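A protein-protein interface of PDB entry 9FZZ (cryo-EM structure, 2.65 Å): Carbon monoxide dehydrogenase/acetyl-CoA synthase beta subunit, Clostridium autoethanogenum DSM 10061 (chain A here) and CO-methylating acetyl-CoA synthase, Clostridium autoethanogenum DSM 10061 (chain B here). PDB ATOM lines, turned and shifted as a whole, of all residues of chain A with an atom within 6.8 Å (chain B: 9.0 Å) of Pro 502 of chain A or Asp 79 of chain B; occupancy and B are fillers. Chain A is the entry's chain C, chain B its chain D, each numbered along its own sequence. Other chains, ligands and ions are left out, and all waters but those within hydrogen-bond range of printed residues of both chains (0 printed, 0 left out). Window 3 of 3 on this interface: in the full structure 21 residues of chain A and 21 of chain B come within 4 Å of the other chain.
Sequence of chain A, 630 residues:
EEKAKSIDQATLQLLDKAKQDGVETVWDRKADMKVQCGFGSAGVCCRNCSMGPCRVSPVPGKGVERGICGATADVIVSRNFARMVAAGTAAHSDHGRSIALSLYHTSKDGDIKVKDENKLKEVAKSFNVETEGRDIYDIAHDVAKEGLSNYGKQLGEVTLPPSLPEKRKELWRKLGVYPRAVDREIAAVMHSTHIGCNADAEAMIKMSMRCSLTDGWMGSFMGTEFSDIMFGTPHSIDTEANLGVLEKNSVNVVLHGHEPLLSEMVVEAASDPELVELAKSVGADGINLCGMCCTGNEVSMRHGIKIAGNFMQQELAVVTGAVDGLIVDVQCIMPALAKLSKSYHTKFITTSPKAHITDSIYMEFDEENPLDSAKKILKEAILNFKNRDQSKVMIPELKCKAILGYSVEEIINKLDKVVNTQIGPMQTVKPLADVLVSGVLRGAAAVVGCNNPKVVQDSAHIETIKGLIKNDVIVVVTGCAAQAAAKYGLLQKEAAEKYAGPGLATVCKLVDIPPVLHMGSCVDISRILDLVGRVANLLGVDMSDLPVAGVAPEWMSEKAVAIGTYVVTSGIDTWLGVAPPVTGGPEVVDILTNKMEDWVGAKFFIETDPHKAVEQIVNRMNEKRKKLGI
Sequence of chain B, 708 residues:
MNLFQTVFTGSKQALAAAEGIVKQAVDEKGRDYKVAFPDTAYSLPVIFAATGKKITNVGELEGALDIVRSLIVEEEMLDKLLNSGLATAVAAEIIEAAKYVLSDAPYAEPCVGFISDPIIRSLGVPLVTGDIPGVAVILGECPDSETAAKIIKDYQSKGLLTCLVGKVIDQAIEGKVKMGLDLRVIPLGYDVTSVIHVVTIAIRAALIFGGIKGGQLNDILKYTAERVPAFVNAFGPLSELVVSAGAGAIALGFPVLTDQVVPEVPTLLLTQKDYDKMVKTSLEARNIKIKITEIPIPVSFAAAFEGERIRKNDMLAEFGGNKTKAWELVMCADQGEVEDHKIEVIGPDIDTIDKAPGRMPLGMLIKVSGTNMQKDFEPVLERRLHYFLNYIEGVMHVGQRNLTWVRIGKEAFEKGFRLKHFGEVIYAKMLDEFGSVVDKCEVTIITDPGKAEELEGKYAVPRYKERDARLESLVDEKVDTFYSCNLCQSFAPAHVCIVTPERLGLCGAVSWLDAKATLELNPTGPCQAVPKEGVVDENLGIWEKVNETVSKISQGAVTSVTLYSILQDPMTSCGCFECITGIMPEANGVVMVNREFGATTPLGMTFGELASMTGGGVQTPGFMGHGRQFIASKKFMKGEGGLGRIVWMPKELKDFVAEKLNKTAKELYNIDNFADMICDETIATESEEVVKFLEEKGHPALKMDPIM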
ATOM      1  N   VAL A 440      18.827  20.112 -10.539  1.00  0.00           N
ATOM      2  CA  VAL A 440      19.865  20.862  -9.834  1.00  0.00           C
ATOM      3  C   VAL A 440      20.551  21.808 -10.808  1.00  0.00           C
ATOM      4  O   VAL A 440      20.850  22.962 -10.477  1.00  0.00           O
ATOM      5  CB  VAL A 440      20.858  19.905  -9.148  1.00  0.00           C
ATOM      6  CG1 VAL A 440      22.051  20.671  -8.562  1.00  0.00           C
ATOM      7  CG2 VAL A 440      20.148  19.107  -8.037  1.00  0.00           C
ATOM      8  N   ILE A 469      25.039  31.431 -15.999  1.00  0.00           N
ATOM      9  CA  ILE A 469      25.520  30.701 -14.821  1.00  0.00           C
ATOM     10  C   ILE A 469      24.787  31.166 -13.566  1.00  0.00           C
ATOM     11  O   ILE A 469      24.606  30.388 -12.628  1.00  0.00           O
ATOM     12  CB  ILE A 469      27.053  30.790 -14.650  1.00  0.00           C
ATOM     13  CG1 ILE A 469      27.508  32.239 -14.357  1.00  0.00           C
ATOM     14  CG2 ILE A 469      27.752  30.113 -15.853  1.00  0.00           C
ATOM     15  CD1 ILE A 469      29.025  32.381 -14.230  1.00  0.00           C
ATOM     16  N   LYS A 470      24.350  32.426 -13.525  1.00  0.00           N
ATOM     17  CA  LYS A 470      23.525  32.869 -12.405  1.00  0.00           C
ATOM     18  C   LYS A 470      22.199  32.110 -12.364  1.00  0.00           C
ATOM     19  O   LYS A 470      21.652  31.887 -11.278  1.00  0.00           O
ATOM     20  CB  LYS A 470      23.301  34.388 -12.497  1.00  0.00           C
ATOM     21  CG  LYS A 470      22.303  34.961 -11.471  1.00  0.00           C
ATOM     22  CD  LYS A 470      22.689  34.587 -10.018  1.00  0.00           C
ATOM     23  CE  LYS A 470      23.986  35.289  -9.571  1.00  0.00           C
ATOM     24  NZ  LYS A 470      23.766  36.770  -9.463  1.00  0.00           N
ATOM     25  N   ASN A 471      21.667  31.698 -13.523  1.00  0.00           N
ATOM     26  CA  ASN A 471      20.426  30.933 -13.614  1.00  0.00           C
ATOM     27  C   ASN A 471      20.650  29.417 -13.544  1.00  0.00           C
ATOM     28  O   ASN A 471      19.807  28.648 -14.023  1.00  0.00           O
ATOM     29  CB  ASN A 471      19.683  31.292 -14.906  1.00  0.00           C
ATOM     30  CG  ASN A 471      19.087  32.689 -14.868  1.00  0.00           C
ATOM     31  OD1 ASN A 471      17.991  32.877 -14.365  1.00  0.00           O
ATOM     32  ND2 ASN A 471      19.818  33.678 -15.386  1.00  0.00           N
ATOM     33  N   ASP A 472      21.759  28.969 -12.947  1.00  0.00           N
ATOM     34  CA  ASP A 472      22.078  27.545 -12.813  1.00  0.00           C
ATOM     35  C   ASP A 472      22.076  26.845 -14.174  1.00  0.00           C
ATOM     36  O   ASP A 472      21.625  25.708 -14.310  1.00  0.00           O
ATOM     37  CB  ASP A 472      21.138  26.831 -11.836  1.00  0.00           C
ATOM     38  CG  ASP A 472      21.513  27.080 -10.380  1.00  0.00           C
ATOM     39  OD1 ASP A 472      22.694  27.394 -10.135  1.00  0.00           O
ATOM     40  OD2 ASP A 472      20.647  26.971  -9.490  1.00  0.00           O
ATOM     41  N   ALA A 500      27.932  32.071  -9.956  1.00  0.00           N
ATOM     42  CA  ALA A 500      26.977  31.008 -10.219  1.00  0.00           C
ATOM     43  C   ALA A 500      25.824  31.026  -9.216  1.00  0.00           C
ATOM     44  O   ALA A 500      25.941  31.545  -8.105  1.00  0.00           O
ATOM     45  CB  ALA A 500      27.676  29.645 -10.183  1.00  0.00           C
ATOM     46  N   GLY A 501      24.684  30.474  -9.644  1.00  0.00           N
ATOM     47  CA  GLY A 501      23.555  30.277  -8.766  1.00  0.00           C
ATOM     48  C   GLY A 501      23.780  29.103  -7.832  1.00  0.00           C
ATOM     49  O   GLY A 501      24.806  28.416  -7.881  1.00  0.00           O
ATOM     50  N   PRO A 502      22.798  28.835  -6.967  1.00  0.00           N
ATOM     51  CA  PRO A 502      23.011  27.796  -5.929  1.00  0.00           C
ATOM     52  C   PRO A 502      23.273  26.401  -6.481  1.00  0.00           C
ATOM     53  O   PRO A 502      24.220  25.736  -6.039  1.00  0.00           O
ATOM     54  CB  PRO A 502      21.721  27.866  -5.088  1.00  0.00           C
ATOM     55  CG  PRO A 502      20.670  28.477  -6.038  1.00  0.00           C
ATOM     56  CD  PRO A 502      21.452  29.444  -6.901  1.00  0.00           C
ATOM     57  N   GLY A 503      22.470  25.938  -7.439  1.00  0.00           N
ATOM     58  CA  GLY A 503      22.659  24.597  -7.967  1.00  0.00           C
ATOM     59  C   GLY A 503      23.983  24.439  -8.689  1.00  0.00           C
ATOM     60  O   GLY A 503      24.694  23.448  -8.505  1.00  0.00           O
ATOM     61  N   LEU A 504      24.331  25.414  -9.527  1.00  0.00           N
ATOM     62  CA  LEU A 504      25.598  25.351 -10.247  1.00  0.00           C
ATOM     63  C   LEU A 504      26.783  25.498  -9.298  1.00  0.00           C
ATOM     64  O   LEU A 504      27.808  24.842  -9.486  1.00  0.00           O
ATOM     65  CB  LEU A 504      25.641  26.409 -11.353  1.00  0.00           C
ATOM     66  CG  LEU A 504      26.885  26.394 -12.267  1.00  0.00           C
ATOM     67  CD1 LEU A 504      27.208  24.997 -12.825  1.00  0.00           C
ATOM     68  CD2 LEU A 504      26.701  27.411 -13.414  1.00  0.00           C
ATOM     69  N   ALA A 505      26.664  26.334  -8.259  1.00  0.00           N
ATOM     70  CA  ALA A 505      27.740  26.450  -7.273  1.00  0.00           C
ATOM     71  C   ALA A 505      27.952  25.127  -6.544  1.00  0.00           C
ATOM     72  O   ALA A 505      29.096  24.704  -6.326  1.00  0.00           O
ATOM     73  CB  ALA A 505      27.445  27.575  -6.274  1.00  0.00           C
ATOM     74  N   THR A 506      26.863  24.456  -6.166  1.00  0.00           N
ATOM     75  CA  THR A 506      26.989  23.142  -5.543  1.00  0.00           C
ATOM     76  C   THR A 506      27.643  22.145  -6.491  1.00  0.00           C
ATOM     77  O   THR A 506      28.550  21.407  -6.091  1.00  0.00           O
ATOM     78  CB  THR A 506      25.610  22.630  -5.117  1.00  0.00           C
ATOM     79  OG1 THR A 506      25.062  23.481  -4.103  1.00  0.00           O
ATOM     80  CG2 THR A 506      25.698  21.202  -4.583  1.00  0.00           C
ATOM     81  N   VAL A 507      27.230  22.135  -7.759  1.00  0.00           N
ATOM     82  CA  VAL A 507      27.820  21.204  -8.723  1.00  0.00           C
ATOM     83  C   VAL A 507      29.308  21.482  -8.892  1.00  0.00           C
ATOM     84  O   VAL A 507      30.131  20.556  -8.907  1.00  0.00           O
ATOM     85  CB  VAL A 507      27.065  21.272 -10.064  1.00  0.00           C
ATOM     86  CG1 VAL A 507      27.803  20.494 -11.155  1.00  0.00           C
ATOM     87  CG2 VAL A 507      25.646  20.725  -9.901  1.00  0.00           C
ATOM     88  N   PHE B   4      11.656  18.478  -7.950  1.00  0.00           N
ATOM     89  CA  PHE B   4      11.246  19.714  -7.292  1.00  0.00           C
ATOM     90  C   PHE B   4       9.761  19.699  -6.967  1.00  0.00           C
ATOM     91  O   PHE B   4       9.351  20.108  -5.874  1.00  0.00           O
ATOM     92  CB  PHE B   4      11.574  20.925  -8.167  1.00  0.00           C
ATOM     93  CG  PHE B   4      13.018  21.343  -8.133  1.00  0.00           C
ATOM     94  CD1 PHE B   4      13.963  20.687  -8.923  1.00  0.00           C
ATOM     95  CD2 PHE B   4      13.436  22.393  -7.311  1.00  0.00           C
ATOM     96  CE1 PHE B   4      15.314  21.063  -8.901  1.00  0.00           C
ATOM     97  CE2 PHE B   4      14.776  22.788  -7.276  1.00  0.00           C
ATOM     98  CZ  PHE B   4      15.726  22.119  -8.073  1.00  0.00           C
ATOM     99  N   VAL B   7       9.033  17.318  -4.046  1.00  0.00           N
ATOM    100  CA  VAL B   7       9.388  17.892  -2.749  1.00  0.00           C
ATOM    101  C   VAL B   7       8.385  18.962  -2.334  1.00  0.00           C
ATOM    102  O   VAL B   7       7.935  18.995  -1.184  1.00  0.00           O
ATOM    103  CB  VAL B   7      10.825  18.443  -2.790  1.00  0.00           C
ATOM    104  CG1 VAL B   7      11.143  19.300  -1.553  1.00  0.00           C
ATOM    105  CG2 VAL B   7      11.819  17.288  -2.913  1.00  0.00           C
ATOM    106  N   PHE B   8       8.002  19.839  -3.266  1.00  0.00           N
ATOM    107  CA  PHE B   8       7.019  20.868  -2.940  1.00  0.00           C
ATOM    108  C   PHE B   8       5.687  20.240  -2.540  1.00  0.00           C
ATOM    109  O   PHE B   8       5.071  20.652  -1.552  1.00  0.00           O
ATOM    110  CB  PHE B   8       6.848  21.832  -4.121  1.00  0.00           C
ATOM    111  CG  PHE B   8       8.083  22.663  -4.432  1.00  0.00           C
ATOM    112  CD1 PHE B   8       8.980  23.029  -3.416  1.00  0.00           C
ATOM    113  CD2 PHE B   8       8.348  23.074  -5.739  1.00  0.00           C
ATOM    114  CE1 PHE B   8      10.134  23.800  -3.695  1.00  0.00           C
ATOM    115  CE2 PHE B   8       9.492  23.844  -6.049  1.00  0.00           C
ATOM    116  CZ  PHE B   8      10.392  24.207  -5.019  1.00  0.00           C
ATOM    117  N   LEU B  71       8.866  28.901   4.324  1.00  0.00           N
ATOM    118  CA  LEU B  71       9.942  28.068   3.802  1.00  0.00           C
ATOM    119  C   LEU B  71       9.576  27.347   2.509  1.00  0.00           C
ATOM    120  O   LEU B  71      10.437  26.689   1.918  1.00  0.00           O
ATOM    121  CB  LEU B  71      10.375  27.038   4.859  1.00  0.00           C
ATOM    122  CG  LEU B  71      11.147  27.607   6.059  1.00  0.00           C
ATOM    123  CD1 LEU B  71      11.427  26.513   7.086  1.00  0.00           C
ATOM    124  CD2 LEU B  71      12.452  28.279   5.610  1.00  0.00           C
ATOM    125  N   ILE B  72       8.333  27.466   2.043  1.00  0.00           N
ATOM    126  CA  ILE B  72       7.898  26.799   0.820  1.00  0.00           C
ATOM    127  C   ILE B  72       7.739  27.854  -0.271  1.00  0.00           C
ATOM    128  O   ILE B  72       6.688  28.492  -0.381  1.00  0.00           O
ATOM    129  CB  ILE B  72       6.599  26.001   1.032  1.00  0.00           C
ATOM    130  CG1 ILE B  72       6.760  25.020   2.207  1.00  0.00           C
ATOM    131  CG2 ILE B  72       6.240  25.246  -0.250  1.00  0.00           C
ATOM    132  CD1 ILE B  72       5.454  24.323   2.619  1.00  0.00           C
ATOM    133  N   VAL B  73       8.781  28.051  -1.079  1.00  0.00           N
ATOM    134  CA  VAL B  73       8.729  28.906  -2.259  1.00  0.00           C
ATOM    135  C   VAL B  73       8.882  28.001  -3.474  1.00  0.00           C
ATOM    136  O   VAL B  73       9.942  27.397  -3.686  1.00  0.00           O
ATOM    137  CB  VAL B  73       9.813  29.990  -2.230  1.00  0.00           C
ATOM    138  CG1 VAL B  73       9.718  30.888  -3.470  1.00  0.00           C
ATOM    139  CG2 VAL B  73       9.690  30.828  -0.961  1.00  0.00           C
ATOM    140  N   GLU B  75       9.754  27.572  -6.540  1.00  0.00           N
ATOM    141  CA  GLU B  75      10.596  27.939  -7.667  1.00  0.00           C
ATOM    142  C   GLU B  75      11.667  26.870  -7.813  1.00  0.00           C
ATOM    143  O   GLU B  75      12.301  26.483  -6.825  1.00  0.00           O
ATOM    144  CB  GLU B  75      11.213  29.328  -7.463  1.00  0.00           C
ATOM    145  CG  GLU B  75      10.142  30.430  -7.424  1.00  0.00           C
ATOM    146  CD  GLU B  75      10.672  31.756  -6.900  1.00  0.00           C
ATOM    147  OE1 GLU B  75      11.816  31.785  -6.418  1.00  0.00           O
ATOM    148  OE2 GLU B  75       9.942  32.766  -6.966  1.00  0.00           O
ATOM    149  N   GLU B  76      11.853  26.373  -9.037  1.00  0.00           N
ATOM    150  CA  GLU B  76      12.713  25.209  -9.273  1.00  0.00           C
ATOM    151  C   GLU B  76      14.183  25.635  -9.304  1.00  0.00           C
ATOM    152  O   GLU B  76      14.845  25.676 -10.344  1.00  0.00           O
ATOM    153  CB  GLU B  76      12.296  24.491 -10.545  1.00  0.00           C
ATOM    154  CG  GLU B  76      10.855  23.965 -10.470  1.00  0.00           C
ATOM    155  CD  GLU B  76      10.566  22.879 -11.492  1.00  0.00           C
ATOM    156  OE1 GLU B  76      11.362  22.732 -12.434  1.00  0.00           O
ATOM    157  OE2 GLU B  76       9.550  22.168 -11.345  1.00  0.00           O
ATOM    158  N   MET B  77      14.693  25.960  -8.112  1.00  0.00           N
ATOM    159  CA  MET B  77      16.112  26.200  -7.887  1.00  0.00           C
ATOM    160  C   MET B  77      16.510  25.454  -6.618  1.00  0.00           C
ATOM    161  O   MET B  77      15.695  25.256  -5.714  1.00  0.00           O
ATOM    162  CB  MET B  77      16.441  27.709  -7.750  1.00  0.00           C
ATOM    163  CG  MET B  77      15.995  28.574  -8.945  1.00  0.00           C
ATOM    164  SD  MET B  77      17.016  28.354 -10.425  1.00  0.00           S
ATOM    165  CE  MET B  77      18.418  29.414 -10.092  1.00  0.00           C
ATOM    166  N   LEU B  78      17.786  25.081  -6.543  1.00  0.00           N
ATOM    167  CA  LEU B  78      18.230  24.158  -5.500  1.00  0.00           C
ATOM    168  C   LEU B  78      17.999  24.732  -4.109  1.00  0.00           C
ATOM    169  O   LEU B  78      17.616  24.002  -3.186  1.00  0.00           O
ATOM    170  CB  LEU B  78      19.703  23.810  -5.709  1.00  0.00           C
ATOM    171  CG  LEU B  78      20.283  22.833  -4.672  1.00  0.00           C
ATOM    172  CD1 LEU B  78      19.550  21.487  -4.711  1.00  0.00           C
ATOM    173  CD2 LEU B  78      21.779  22.641  -4.898  1.00  0.00           C
ATOM    174  N   ASP B  79      18.214  26.037  -3.934  1.00  0.00           N
ATOM    175  CA  ASP B  79      18.037  26.643  -2.617  1.00  0.00           C
ATOM    176  C   ASP B  79      16.589  26.520  -2.147  1.00  0.00           C
ATOM    177  O   ASP B  79      16.339  26.203  -0.979  1.00  0.00           O
ATOM    178  CB  ASP B  79      18.499  28.104  -2.633  1.00  0.00           C
ATOM    179  CG  ASP B  79      17.779  28.938  -3.679  1.00  0.00           C
ATOM    180  OD1 ASP B  79      17.761  28.518  -4.854  1.00  0.00           O
ATOM    181  OD2 ASP B  79      17.214  29.991  -3.329  1.00  0.00           O
ATOM    182  N   LYS B  80      15.617  26.720  -3.049  1.00  0.00           N
ATOM    183  CA  LYS B  80      14.211  26.577  -2.664  1.00  0.00           C
ATOM    184  C   LYS B  80      13.882  25.137  -2.293  1.00  0.00           C
ATOM    185  O   LYS B  80      13.082  24.889  -1.387  1.00  0.00           O
ATOM    186  CB  LYS B  80      13.270  27.042  -3.783  1.00  0.00           C
ATOM    187  CG  LYS B  80      13.174  28.563  -3.934  1.00  0.00           C
ATOM    188  CD  LYS B  80      14.323  29.093  -4.794  1.00  0.00           C
ATOM    189  CE  LYS B  80      14.380  30.631  -4.792  1.00  0.00           C
ATOM    190  NZ  LYS B  80      14.709  31.179  -3.432  1.00  0.00           N
ATOM    191  N   LEU B  81      14.473  24.175  -3.001  1.00  0.00           N
ATOM    192  CA  LEU B  81      14.247  22.770  -2.682  1.00  0.00           C
ATOM    193  C   LEU B  81      14.756  22.439  -1.286  1.00  0.00           C
ATOM    194  O   LEU B  81      14.101  21.709  -0.533  1.00  0.00           O
ATOM    195  CB  LEU B  81      14.911  21.893  -3.749  1.00  0.00           C
ATOM    196  CG  LEU B  81      14.755  20.371  -3.630  1.00  0.00           C
ATOM    197  CD1 LEU B  81      14.767  19.724  -5.017  1.00  0.00           C
ATOM    198  CD2 LEU B  81      15.863  19.782  -2.758  1.00  0.00           C
ATOM    199  N   LEU B  82      15.936  22.946  -0.924  1.00  0.00           N
ATOM    200  CA  LEU B  82      16.468  22.712   0.417  1.00  0.00           C
ATOM    201  C   LEU B  82      15.626  23.414   1.478  1.00  0.00           C
ATOM    202  O   LEU B  82      15.377  22.856   2.552  1.00  0.00           O
ATOM    203  CB  LEU B  82      17.934  23.154   0.497  1.00  0.00           C
ATOM    204  CG  LEU B  82      18.865  22.462  -0.518  1.00  0.00           C
ATOM    205  CD1 LEU B  82      20.265  23.069  -0.465  1.00  0.00           C
ATOM    206  CD2 LEU B  82      18.942  20.950  -0.307  1.00  0.00           C
ATOM    207  N   ASN B  83      15.159  24.637   1.192  1.00  0.00           N
ATOM    208  CA  ASN B  83      14.263  25.324   2.119  1.00  0.00           C
ATOM    209  C   ASN B  83      12.950  24.569   2.277  1.00  0.00           C
ATOM    210  O   ASN B  83      12.389  24.512   3.376  1.00  0.00           O
ATOM    211  CB  ASN B  83      13.990  26.752   1.641  1.00  0.00           C
ATOM    212  CG  ASN B  83      15.166  27.683   1.862  1.00  0.00           C
ATOM    213  OD1 ASN B  83      15.851  27.581   2.870  1.00  0.00           O
ATOM    214  ND2 ASN B  83      15.413  28.583   0.918  1.00  0.00           N
ATOM    215  N   SER B  84      12.441  23.998   1.188  1.00  0.00           N
ATOM    216  CA  SER B  84      11.214  23.217   1.271  1.00  0.00           C
ATOM    217  C   SER B  84      11.426  21.937   2.075  1.00  0.00           C
ATOM    218  O   SER B  84      10.528  21.502   2.804  1.00  0.00           O
ATOM    219  CB  SER B  84      10.699  22.917  -0.140  1.00  0.00           C
ATOM    220  OG  SER B  84       9.499  22.159  -0.100  1.00  0.00           O
ATOM    221  N   GLY B  85      12.605  21.321   1.964  1.00  0.00           N
ATOM    222  CA  GLY B  85      12.912  20.201   2.836  1.00  0.00           C
ATOM    223  C   GLY B  85      12.909  20.608   4.296  1.00  0.00           C
ATOM    224  O   GLY B  85      12.397  19.888   5.155  1.00  0.00           O
ATOM    225  N   LEU B  86      13.457  21.787   4.594  1.00  0.00           N
ATOM    226  CA  LEU B  86      13.415  22.297   5.961  1.00  0.00           C
ATOM    227  C   LEU B  86      11.991  22.628   6.391  1.00  0.00           C
ATOM    228  O   LEU B  86      11.667  22.535   7.576  1.00  0.00           O
ATOM    229  CB  LEU B  86      14.322  23.523   6.090  1.00  0.00           C
ATOM    230  CG  LEU B  86      15.815  23.218   5.878  1.00  0.00           C
ATOM    231  CD1 LEU B  86      16.630  24.500   5.902  1.00  0.00           C
ATOM    232  CD2 LEU B  86      16.340  22.228   6.928  1.00  0.00           C
ATOM    233  N   ALA B  87      11.129  23.008   5.446  1.00  0.00           N
ATOM    234  CA  ALA B  87       9.729  23.235   5.785  1.00  0.00           C
ATOM    235  C   ALA B  87       9.071  21.948   6.266  1.00  0.00           C
ATOM    236  O   ALA B  87       8.293  21.961   7.226  1.00  0.00           O
ATOM    237  CB  ALA B  87       8.983  23.810   4.579  1.00  0.00           C
ATOM    238  N   LEU B 221      23.379  24.274   9.955  1.00  0.00           N
ATOM    239  CA  LEU B 221      23.401  23.384   8.795  1.00  0.00           C
ATOM    240  C   LEU B 221      24.826  23.037   8.392  1.00  0.00           C
ATOM    241  O   LEU B 221      25.114  21.893   8.024  1.00  0.00           O
ATOM    242  CB  LEU B 221      22.648  24.015   7.621  1.00  0.00           C
ATOM    243  CG  LEU B 221      21.155  24.271   7.876  1.00  0.00           C
ATOM    244  CD1 LEU B 221      20.514  24.878   6.639  1.00  0.00           C
ATOM    245  CD2 LEU B 221      20.414  23.000   8.296  1.00  0.00           C
ATOM    246  N   ALA B 247      14.486  15.612   1.414  1.00  0.00           N
ATOM    247  CA  ALA B 247      15.070  16.902   1.066  1.00  0.00           C
ATOM    248  C   ALA B 247      15.485  17.653   2.325  1.00  0.00           C
ATOM    249  O   ALA B 247      16.446  18.427   2.301  1.00  0.00           O
ATOM    250  CB  ALA B 247      14.086  17.729   0.225  1.00  0.00           C
ATOM    251  N   ALA B 251      19.110  18.852   3.171  1.00  0.00           N
ATOM    252  CA  ALA B 251      19.361  20.214   3.633  1.00  0.00           C
ATOM    253  C   ALA B 251      20.329  20.240   4.809  1.00  0.00           C
ATOM    254  O   ALA B 251      21.096  21.194   4.957  1.00  0.00           O
ATOM    255  CB  ALA B 251      18.043  20.905   4.007  1.00  0.00           C
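OD2 of Asp 79 of chain B lies within salt-bridge range of NZ of Lys 80 of chain B (2.8 Å). The backbone carbonyl oxygen (O) of Asp 79 of chain B is in hydrogen-bond range of the side-chain amide nitrogen (ND2) of Asn 83 of chain B (3.2 Å). The side-chain carboxylate (OD2) of Asp 472 of chain A lies within hydrogen-bond range of the backbone NH (N) of Gly 503 of chain A, at 2.9 Å. The side-chain carboxylate (OD1) of Asp 472 of chain A lies within hydrogen-bond range of the backbone NH (N) of Leu 504 of chain A (2.6 Å). The side-chain hydroxyl of Thr 506 of chain A sits at hydrogen-bond distance from the backbone carbonyl oxygen of Pro 502 of chain A, at 3.1 Å.
Among the printed residues, pairs that only touch across the chains: Val 440 of chain A with Phe 4 of chain B, Asp 472 of chain A with Met 77 of chain B, Pro 502 of chain A with Asp 79 of chain B, Gly 503 of chain A with Leu 78 of chain B and Thr 506 of chain A with Leu 78 of chain B.
Printed residues of chain B within 4 Å of Val 440 of chain A: Phe 4 (3.99 Å). Ile 469 of chain A touches none of the printed residues of chain B. No residue of chain B comes within 4 Å of Gly 501 of chain A. Printed residues of chain B within 4 Å of Pro 502 of chain A: Asp 79. Of the printed residues of chain B, Thr 506 of chain A touches Leu 78. Val 507 of chain A touches none of the printed residues of chain B. Printed residues of chain A within 4 Å of Phe 4 of chain B: Val 440. Asp 79 of chain B touches just one residue of chain A: Pro 502 (3.1 Å).
Of the 13 printed residues of chain A, 5 touch a printed residue of chain B. Hydrophobic or aromatic side chains of chain A that line the printed part of chain B: Pro 502. Of the 22 printed residues of chain B, 4 touch a printed residue of chain A. Printed residues of chain B that touch a printed residue of chain A: Phe 4, Met 77, Leu 78 and Asp 79. Among the printed residues, no Asp or Glu carboxylate lies within 4 Å of a Lys or Arg side-chain nitrogen of the other chain.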
